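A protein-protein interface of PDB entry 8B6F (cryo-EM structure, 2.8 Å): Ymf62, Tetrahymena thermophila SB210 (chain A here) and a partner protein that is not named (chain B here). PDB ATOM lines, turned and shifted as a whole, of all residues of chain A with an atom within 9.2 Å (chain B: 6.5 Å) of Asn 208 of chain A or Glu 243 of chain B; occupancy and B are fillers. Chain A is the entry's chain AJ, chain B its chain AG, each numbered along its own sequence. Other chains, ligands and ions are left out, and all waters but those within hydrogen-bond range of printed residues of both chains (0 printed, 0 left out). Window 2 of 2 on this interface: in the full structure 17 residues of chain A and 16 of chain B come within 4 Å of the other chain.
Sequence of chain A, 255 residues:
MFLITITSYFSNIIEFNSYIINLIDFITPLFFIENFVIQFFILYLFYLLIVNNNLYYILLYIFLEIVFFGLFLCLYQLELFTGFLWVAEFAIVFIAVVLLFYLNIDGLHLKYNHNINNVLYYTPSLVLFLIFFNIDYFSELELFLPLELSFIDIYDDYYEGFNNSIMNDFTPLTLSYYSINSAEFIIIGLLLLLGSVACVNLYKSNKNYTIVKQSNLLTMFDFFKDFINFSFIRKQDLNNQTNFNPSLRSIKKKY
The backbone carbonyl oxygen of Val 212 of chain A lies within hydrogen-bond range of a ring nitrogen (ND1) of His 242 of chain B, at 3.3 Å.
The backbone carbonyl oxygen of Lys 204 of chain A sits close to the side-chain amide nitrogen of Asn 208 of chain A, 3.3 Å away.
Among the printed residues, merely in contact across the chains: Asn 208 of chain A with Glu 243 of chain B, Ile 211 of chain A with Glu 243 of chain B, Ser 215 of chain A with Leu 245 of chain B and Ser 215 of chain A with Ala 246 of chain B.
Asn 208 of chain A touches just one residue of chain B: Glu 243. Of the printed residues of chain B, Ile 211 of chain A touches Glu 243 (3.8 Å). Of the printed residues of chain B, Val 212 of chain A touches His 242. Gln 214 of chain A touches none of the printed residues of chain B. Of the printed residues of chain A, His 242 of chain B touches Val 212 (3.3 Å). Glu 243 of chain B touches two residues of chain A. Of the printed residues of chain A, Leu 245 of chain B touches Ser 215. Gln 248 of chain B touches none of the printed residues of chain A. The nearest residue of chain B that does not touch Asn 208 of chain A is His 242 of chain B (6.1 Å).
Of the 9 printed residues of chain B, 4 touch a printed residue of chain A. Hydrophobic or aromatic side chains of chain B within 4 Å of the printed part of chain A: His 242 and Leu 245. Along chain A the printed residues that touch a printed residue of chain B span positions 208 to 215. Among the printed residues, 5 pairs touch across the chains. Among the printed residues, no Asp or Glu carboxylate lies within 4 Å of a Lys or Arg side-chain nitrogen of the other chain.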
ATOM      1  N   VAL A 200      -5.578  25.745 -21.241  1.00  0.00           N
ATOM      2  CA  VAL A 200      -4.147  25.457 -21.249  1.00  0.00           C
ATOM      3  C   VAL A 200      -3.746  24.715 -19.981  1.00  0.00           C
ATOM      4  O   VAL A 200      -2.986  23.741 -20.028  1.00  0.00           O
ATOM      5  CB  VAL A 200      -3.345  26.759 -21.421  1.00  0.00           C
ATOM      6  CG1 VAL A 200      -1.856  26.513 -21.224  1.00  0.00           C
ATOM      7  CG2 VAL A 200      -3.605  27.359 -22.789  1.00  0.00           C
ATOM      8  N   ASN A 201      -4.243  25.165 -18.830  1.00  0.00           N
ATOM      9  CA  ASN A 201      -3.898  24.509 -17.573  1.00  0.00           C
ATOM     10  C   ASN A 201      -4.440  23.087 -17.522  1.00  0.00           C
ATOM     11  O   ASN A 201      -3.785  22.186 -16.986  1.00  0.00           O
ATOM     12  CB  ASN A 201      -4.414  25.334 -16.399  1.00  0.00           C
ATOM     13  CG  ASN A 201      -3.591  26.582 -16.169  1.00  0.00           C
ATOM     14  OD1 ASN A 201      -2.641  26.576 -15.390  1.00  0.00           O
ATOM     15  ND2 ASN A 201      -3.944  27.658 -16.860  1.00  0.00           N
ATOM     16  N   LEU A 202      -5.640  22.867 -18.062  1.00  0.00           N
ATOM     17  CA  LEU A 202      -6.188  21.515 -18.112  1.00  0.00           C
ATOM     18  C   LEU A 202      -5.349  20.619 -19.012  1.00  0.00           C
ATOM     19  O   LEU A 202      -5.141  19.440 -18.705  1.00  0.00           O
ATOM     20  CB  LEU A 202      -7.642  21.553 -18.581  1.00  0.00           C
ATOM     21  CG  LEU A 202      -8.374  20.210 -18.665  1.00  0.00           C
ATOM     22  CD1 LEU A 202      -8.226  19.403 -17.387  1.00  0.00           C
ATOM     23  CD2 LEU A 202      -9.839  20.451 -18.953  1.00  0.00           C
ATOM     24  N   TYR A 203      -4.864  21.158 -20.130  1.00  0.00           N
ATOM     25  CA  TYR A 203      -3.965  20.396 -20.988  1.00  0.00           C
ATOM     26  C   TYR A 203      -2.694  20.004 -20.243  1.00  0.00           C
ATOM     27  O   TYR A 203      -2.234  18.861 -20.343  1.00  0.00           O
ATOM     28  CB  TYR A 203      -3.629  21.213 -22.233  1.00  0.00           C
ATOM     29  CG  TYR A 203      -2.561  20.603 -23.108  1.00  0.00           C
ATOM     30  CD1 TYR A 203      -2.880  19.650 -24.064  1.00  0.00           C
ATOM     31  CD2 TYR A 203      -1.235  20.992 -22.987  1.00  0.00           C
ATOM     32  CE1 TYR A 203      -1.907  19.094 -24.868  1.00  0.00           C
ATOM     33  CE2 TYR A 203      -0.255  20.445 -23.784  1.00  0.00           C
ATOM     34  CZ  TYR A 203      -0.597  19.496 -24.723  1.00  0.00           C
ATOM     35  OH  TYR A 203       0.378  18.948 -25.521  1.00  0.00           O
ATOM     36  N   LYS A 204      -2.109  20.941 -19.493  1.00  0.00           N
ATOM     37  CA  LYS A 204      -0.913  20.625 -18.721  1.00  0.00           C
ATOM     38  C   LYS A 204      -1.206  19.568 -17.665  1.00  0.00           C
ATOM     39  O   LYS A 204      -0.392  18.670 -17.431  1.00  0.00           O
ATOM     40  CB  LYS A 204      -0.350  21.890 -18.074  1.00  0.00           C
ATOM     41  CG  LYS A 204       0.193  22.898 -19.077  1.00  0.00           C
ATOM     42  CD  LYS A 204       0.903  24.057 -18.391  1.00  0.00           C
ATOM     43  CE  LYS A 204      -0.059  24.903 -17.571  1.00  0.00           C
ATOM     44  NZ  LYS A 204       0.618  26.081 -16.956  1.00  0.00           N
ATOM     45  N   SER A 205      -2.362  19.668 -17.004  1.00  0.00           N
ATOM     46  CA  SER A 205      -2.731  18.670 -16.006  1.00  0.00           C
ATOM     47  C   SER A 205      -2.881  17.294 -16.638  1.00  0.00           C
ATOM     48  O   SER A 205      -2.465  16.285 -16.056  1.00  0.00           O
ATOM     49  CB  SER A 205      -4.027  19.079 -15.306  1.00  0.00           C
ATOM     50  OG  SER A 205      -3.880  20.329 -14.655  1.00  0.00           O
ATOM     51  N   ASN A 206      -3.482  17.230 -17.825  1.00  0.00           N
ATOM     52  CA  ASN A 206      -3.571  15.962 -18.538  1.00  0.00           C
ATOM     53  C   ASN A 206      -2.185  15.419 -18.861  1.00  0.00           C
ATOM     54  O   ASN A 206      -1.940  14.212 -18.747  1.00  0.00           O
ATOM     55  CB  ASN A 206      -4.390  16.146 -19.816  1.00  0.00           C
ATOM     56  CG  ASN A 206      -4.539  14.863 -20.603  1.00  0.00           C
ATOM     57  OD1 ASN A 206      -5.455  14.079 -20.366  1.00  0.00           O
ATOM     58  ND2 ASN A 206      -3.641  14.648 -21.557  1.00  0.00           N
ATOM     59  N   LYS A 207      -1.264  16.295 -19.264  1.00  0.00           N
ATOM     60  CA  LYS A 207       0.092  15.858 -19.578  1.00  0.00           C
ATOM     61  C   LYS A 207       0.798  15.301 -18.348  1.00  0.00           C
ATOM     62  O   LYS A 207       1.585  14.355 -18.453  1.00  0.00           O
ATOM     63  CB  LYS A 207       0.894  17.017 -20.172  1.00  0.00           C
ATOM     64  CG  LYS A 207       0.857  17.082 -21.689  1.00  0.00           C
ATOM     65  CD  LYS A 207       1.690  15.971 -22.311  1.00  0.00           C
ATOM     66  CE  LYS A 207       1.665  16.042 -23.828  1.00  0.00           C
ATOM     67  NZ  LYS A 207       0.298  15.830 -24.380  1.00  0.00           N
ATOM     68  N   ASN A 208       0.548  15.882 -17.175  1.00  0.00           N
ATOM     69  CA  ASN A 208       1.295  15.488 -15.986  1.00  0.00           C
ATOM     70  C   ASN A 208       1.180  13.998 -15.685  1.00  0.00           C
ATOM     71  O   ASN A 208       2.084  13.439 -15.056  1.00  0.00           O
ATOM     72  CB  ASN A 208       0.825  16.291 -14.771  1.00  0.00           C
ATOM     73  CG  ASN A 208       1.282  17.737 -14.812  1.00  0.00           C
ATOM     74  OD1 ASN A 208       2.349  18.049 -15.339  1.00  0.00           O
ATOM     75  ND2 ASN A 208       0.475  18.628 -14.247  1.00  0.00           N
ATOM     76  N   TYR A 209       0.113  13.338 -16.137  1.00  0.00           N
ATOM     77  CA  TYR A 209      -0.069  11.923 -15.824  1.00  0.00           C
ATOM     78  C   TYR A 209       1.075  11.077 -16.366  1.00  0.00           C
ATOM     79  O   TYR A 209       1.569  10.176 -15.681  1.00  0.00           O
ATOM     80  CB  TYR A 209      -1.408  11.430 -16.373  1.00  0.00           C
ATOM     81  CG  TYR A 209      -2.579  11.766 -15.481  1.00  0.00           C
ATOM     82  CD1 TYR A 209      -2.955  10.917 -14.449  1.00  0.00           C
ATOM     83  CD2 TYR A 209      -3.306  12.933 -15.668  1.00  0.00           C
ATOM     84  CE1 TYR A 209      -4.022  11.220 -13.629  1.00  0.00           C
ATOM     85  CE2 TYR A 209      -4.374  13.246 -14.852  1.00  0.00           C
ATOM     86  CZ  TYR A 209      -4.727  12.385 -13.835  1.00  0.00           C
ATOM     87  OH  TYR A 209      -5.789  12.688 -13.019  1.00  0.00           O
ATOM     88  N   THR A 210       1.507  11.345 -17.599  1.00  0.00           N
ATOM     89  CA  THR A 210       2.636  10.613 -18.160  1.00  0.00           C
ATOM     90  C   THR A 210       3.966  11.060 -17.568  1.00  0.00           C
ATOM     91  O   THR A 210       4.946  10.315 -17.648  1.00  0.00           O
ATOM     92  CB  THR A 210       2.671  10.751 -19.687  1.00  0.00           C
ATOM     93  OG1 THR A 210       3.850  10.119 -20.201  1.00  0.00           O
ATOM     94  CG2 THR A 210       2.656  12.206 -20.119  1.00  0.00           C
ATOM     95  N   ILE A 211       4.021  12.252 -16.970  1.00  0.00           N
ATOM     96  CA  ILE A 211       5.255  12.735 -16.358  1.00  0.00           C
ATOM     97  C   ILE A 211       5.479  12.155 -14.967  1.00  0.00           C
ATOM     98  O   ILE A 211       6.615  12.166 -14.479  1.00  0.00           O
ATOM     99  CB  ILE A 211       5.247  14.273 -16.275  1.00  0.00           C
ATOM    100  CG1 ILE A 211       5.052  14.886 -17.665  1.00  0.00           C
ATOM    101  CG2 ILE A 211       6.537  14.790 -15.645  1.00  0.00           C
ATOM    102  CD1 ILE A 211       4.838  16.390 -17.652  1.00  0.00           C
ATOM    103  N   VAL A 212       4.433  11.637 -14.319  1.00  0.00           N
ATOM    104  CA  VAL A 212       4.541  11.232 -12.918  1.00  0.00           C
ATOM    105  C   VAL A 212       5.696  10.258 -12.717  1.00  0.00           C
ATOM    106  O   VAL A 212       6.523  10.428 -11.813  1.00  0.00           O
ATOM    107  CB  VAL A 212       3.213  10.624 -12.433  1.00  0.00           C
ATOM    108  CG1 VAL A 212       3.350  10.062 -11.025  1.00  0.00           C
ATOM    109  CG2 VAL A 212       2.104  11.649 -12.492  1.00  0.00           C
ATOM    110  N   LYS A 213       5.772   9.222 -13.548  1.00  0.00           N
ATOM    111  CA  LYS A 213       6.683   8.111 -13.300  1.00  0.00           C
ATOM    112  C   LYS A 213       7.996   8.214 -14.064  1.00  0.00           C
ATOM    113  O   LYS A 213       8.835   7.318 -13.940  1.00  0.00           O
ATOM    114  CB  LYS A 213       5.997   6.787 -13.645  1.00  0.00           C
ATOM    115  CG  LYS A 213       4.893   6.410 -12.671  1.00  0.00           C
ATOM    116  CD  LYS A 213       4.382   5.007 -12.922  1.00  0.00           C
ATOM    117  CE  LYS A 213       3.373   4.599 -11.863  1.00  0.00           C
ATOM    118  NZ  LYS A 213       2.861   3.217 -12.086  1.00  0.00           N
ATOM    119  N   GLN A 214       8.201   9.272 -14.849  1.00  0.00           N
ATOM    120  CA  GLN A 214       9.434   9.377 -15.623  1.00  0.00           C
ATOM    121  C   GLN A 214      10.649   9.497 -14.711  1.00  0.00           C
ATOM    122  O   GLN A 214      11.718   8.958 -15.015  1.00  0.00           O
ATOM    123  CB  GLN A 214       9.359  10.569 -16.575  1.00  0.00           C
ATOM    124  CG  GLN A 214       8.180  10.512 -17.520  1.00  0.00           C
ATOM    125  CD  GLN A 214       8.215  11.615 -18.552  1.00  0.00           C
ATOM    126  OE1 GLN A 214       9.199  12.343 -18.664  1.00  0.00           O
ATOM    127  NE2 GLN A 214       7.137  11.746 -19.316  1.00  0.00           N
ATOM    128  N   SER A 215      10.503  10.203 -13.589  1.00  0.00           N
ATOM    129  CA  SER A 215      11.615  10.356 -12.658  1.00  0.00           C
ATOM    130  C   SER A 215      12.109   9.005 -12.160  1.00  0.00           C
ATOM    131  O   SER A 215      13.308   8.710 -12.213  1.00  0.00           O
ATOM    132  CB  SER A 215      11.191  11.234 -11.481  1.00  0.00           C
ATOM    133  OG  SER A 215      12.216  11.298 -10.506  1.00  0.00           O
ATOM    134  N   LEU A 218      13.794   6.897 -15.032  1.00  0.00           N
ATOM    135  CA  LEU A 218      15.162   7.286 -15.352  1.00  0.00           C
ATOM    136  C   LEU A 218      16.107   7.044 -14.184  1.00  0.00           C
ATOM    137  O   LEU A 218      17.311   6.861 -14.391  1.00  0.00           O
ATOM    138  CB  LEU A 218      15.205   8.753 -15.775  1.00  0.00           C
ATOM    139  CG  LEU A 218      14.402   9.105 -17.031  1.00  0.00           C
ATOM    140  CD1 LEU A 218      14.417  10.603 -17.271  1.00  0.00           C
ATOM    141  CD2 LEU A 218      14.938   8.366 -18.247  1.00  0.00           C
ATOM    142  N   TYR B 240       9.763  19.895  -4.129  1.00  0.00           N
ATOM    143  CA  TYR B 240       9.870  19.533  -5.534  1.00  0.00           C
ATOM    144  C   TYR B 240       8.769  18.548  -5.909  1.00  0.00           C
ATOM    145  O   TYR B 240       8.343  17.719  -5.102  1.00  0.00           O
ATOM    146  CB  TYR B 240      11.241  18.918  -5.835  1.00  0.00           C
ATOM    147  CG  TYR B 240      12.366  19.918  -6.022  1.00  0.00           C
ATOM    148  CD1 TYR B 240      12.147  21.148  -6.633  1.00  0.00           C
ATOM    149  CD2 TYR B 240      13.653  19.622  -5.594  1.00  0.00           C
ATOM    150  CE1 TYR B 240      13.174  22.055  -6.803  1.00  0.00           C
ATOM    151  CE2 TYR B 240      14.686  20.523  -5.760  1.00  0.00           C
ATOM    152  CZ  TYR B 240      14.441  21.735  -6.366  1.00  0.00           C
ATOM    153  OH  TYR B 240      15.469  22.634  -6.533  1.00  0.00           O
ATOM    154  N   ASP B 241       8.308  18.647  -7.150  1.00  0.00           N
ATOM    155  CA  ASP B 241       7.234  17.817  -7.675  1.00  0.00           C
ATOM    156  C   ASP B 241       7.799  16.798  -8.662  1.00  0.00           C
ATOM    157  O   ASP B 241       8.999  16.761  -8.939  1.00  0.00           O
ATOM    158  CB  ASP B 241       6.159  18.686  -8.331  1.00  0.00           C
ATOM    159  CG  ASP B 241       6.725  19.618  -9.381  1.00  0.00           C
ATOM    160  OD1 ASP B 241       7.896  20.029  -9.243  1.00  0.00           O
ATOM    161  OD2 ASP B 241       6.002  19.937 -10.347  1.00  0.00           O
ATOM    162  N   HIS B 242       6.909  15.958  -9.193  1.00  0.00           N
ATOM    163  CA  HIS B 242       7.336  14.916 -10.122  1.00  0.00           C
ATOM    164  C   HIS B 242       7.977  15.516 -11.365  1.00  0.00           C
ATOM    165  O   HIS B 242       8.984  15.001 -11.863  1.00  0.00           O
ATOM    166  CB  HIS B 242       6.148  14.035 -10.507  1.00  0.00           C
ATOM    167  CG  HIS B 242       5.607  13.223  -9.373  1.00  0.00           C
ATOM    168  ND1 HIS B 242       6.174  12.032  -8.974  1.00  0.00           N
ATOM    169  CD2 HIS B 242       4.552  13.430  -8.551  1.00  0.00           C
ATOM    170  CE1 HIS B 242       5.492  11.540  -7.957  1.00  0.00           C
ATOM    171  NE2 HIS B 242       4.502  12.368  -7.680  1.00  0.00           N
ATOM    172  N   GLU B 243       7.403  16.600 -11.887  1.00  0.00           N
ATOM    173  CA  GLU B 243       7.979  17.237 -13.066  1.00  0.00           C
ATOM    174  C   GLU B 243       9.375  17.774 -12.776  1.00  0.00           C
ATOM    175  O   GLU B 243      10.281  17.644 -13.606  1.00  0.00           O
ATOM    176  CB  GLU B 243       7.062  18.356 -13.556  1.00  0.00           C
ATOM    177  CG  GLU B 243       7.419  18.862 -14.938  1.00  0.00           C
ATOM    178  CD  GLU B 243       6.405  19.848 -15.475  1.00  0.00           C
ATOM    179  OE1 GLU B 243       5.447  20.170 -14.744  1.00  0.00           O
ATOM    180  OE2 GLU B 243       6.566  20.298 -16.628  1.00  0.00           O
ATOM    181  N   SER B 244       9.569  18.382 -11.605  1.00  0.00           N
ATOM    182  CA  SER B 244      10.890  18.892 -11.254  1.00  0.00           C
ATOM    183  C   SER B 244      11.902  17.763 -11.130  1.00  0.00           C
ATOM    184  O   SER B 244      13.038  17.883 -11.600  1.00  0.00           O
ATOM    185  CB  SER B 244      10.819  19.686  -9.950  1.00  0.00           C
ATOM    186  OG  SER B 244       9.981  20.820 -10.086  1.00  0.00           O
ATOM    187  N   LEU B 245      11.511  16.655 -10.496  1.00  0.00           N
ATOM    188  CA  LEU B 245      12.417  15.517 -10.377  1.00  0.00           C
ATOM    189  C   LEU B 245      12.759  14.941 -11.744  1.00  0.00           C
ATOM    190  O   LEU B 245      13.919  14.612 -12.014  1.00  0.00           O
ATOM    191  CB  LEU B 245      11.800  14.443  -9.483  1.00  0.00           C
ATOM    192  CG  LEU B 245      11.480  14.874  -8.051  1.00  0.00           C
ATOM    193  CD1 LEU B 245      10.713  13.780  -7.333  1.00  0.00           C
ATOM    194  CD2 LEU B 245      12.750  15.221  -7.294  1.00  0.00           C
ATOM    195  N   ALA B 246      11.764  14.818 -12.623  1.00  0.00           N
ATOM    196  CA  ALA B 246      12.028  14.327 -13.971  1.00  0.00           C
ATOM    197  C   ALA B 246      12.987  15.248 -14.711  1.00  0.00           C
ATOM    198  O   ALA B 246      13.891  14.782 -15.413  1.00  0.00           O
ATOM    199  CB  ALA B 246      10.717  14.187 -14.743  1.00  0.00           C
ATOM    200  N   LEU B 247      12.813  16.561 -14.556  1.00  0.00           N
ATOM    201  CA  LEU B 247      13.727  17.509 -15.184  1.00  0.00           C
ATOM    202  C   LEU B 247      15.138  17.360 -14.637  1.00  0.00           C
ATOM    203  O   LEU B 247      16.115  17.447 -15.390  1.00  0.00           O
ATOM    204  CB  LEU B 247      13.223  18.937 -14.982  1.00  0.00           C
ATOM    205  CG  LEU B 247      11.965  19.341 -15.748  1.00  0.00           C
ATOM    206  CD1 LEU B 247      11.470  20.699 -15.286  1.00  0.00           C
ATOM    207  CD2 LEU B 247      12.247  19.358 -17.241  1.00  0.00           C
ATOM    208  N   GLN B 248      15.272  17.135 -13.329  1.00  0.00           N
ATOM    209  CA  GLN B 248      16.598  16.918 -12.759  1.00  0.00           C
ATOM    210  C   GLN B 248      17.268  15.710 -13.400  1.00  0.00           C
ATOM    211  O   GLN B 248      18.437  15.770 -13.795  1.00  0.00           O
ATOM    212  CB  GLN B 248      16.496  16.734 -11.245  1.00  0.00           C
ATOM    213  CG  GLN B 248      16.136  18.001 -10.497  1.00  0.00           C
ATOM    214  CD  GLN B 248      15.997  17.772  -9.010  1.00  0.00           C
ATOM    215  OE1 GLN B 248      16.266  16.683  -8.509  1.00  0.00           O
ATOM    216  NE2 GLN B 248      15.572  18.803  -8.293  1.00  0.00           N
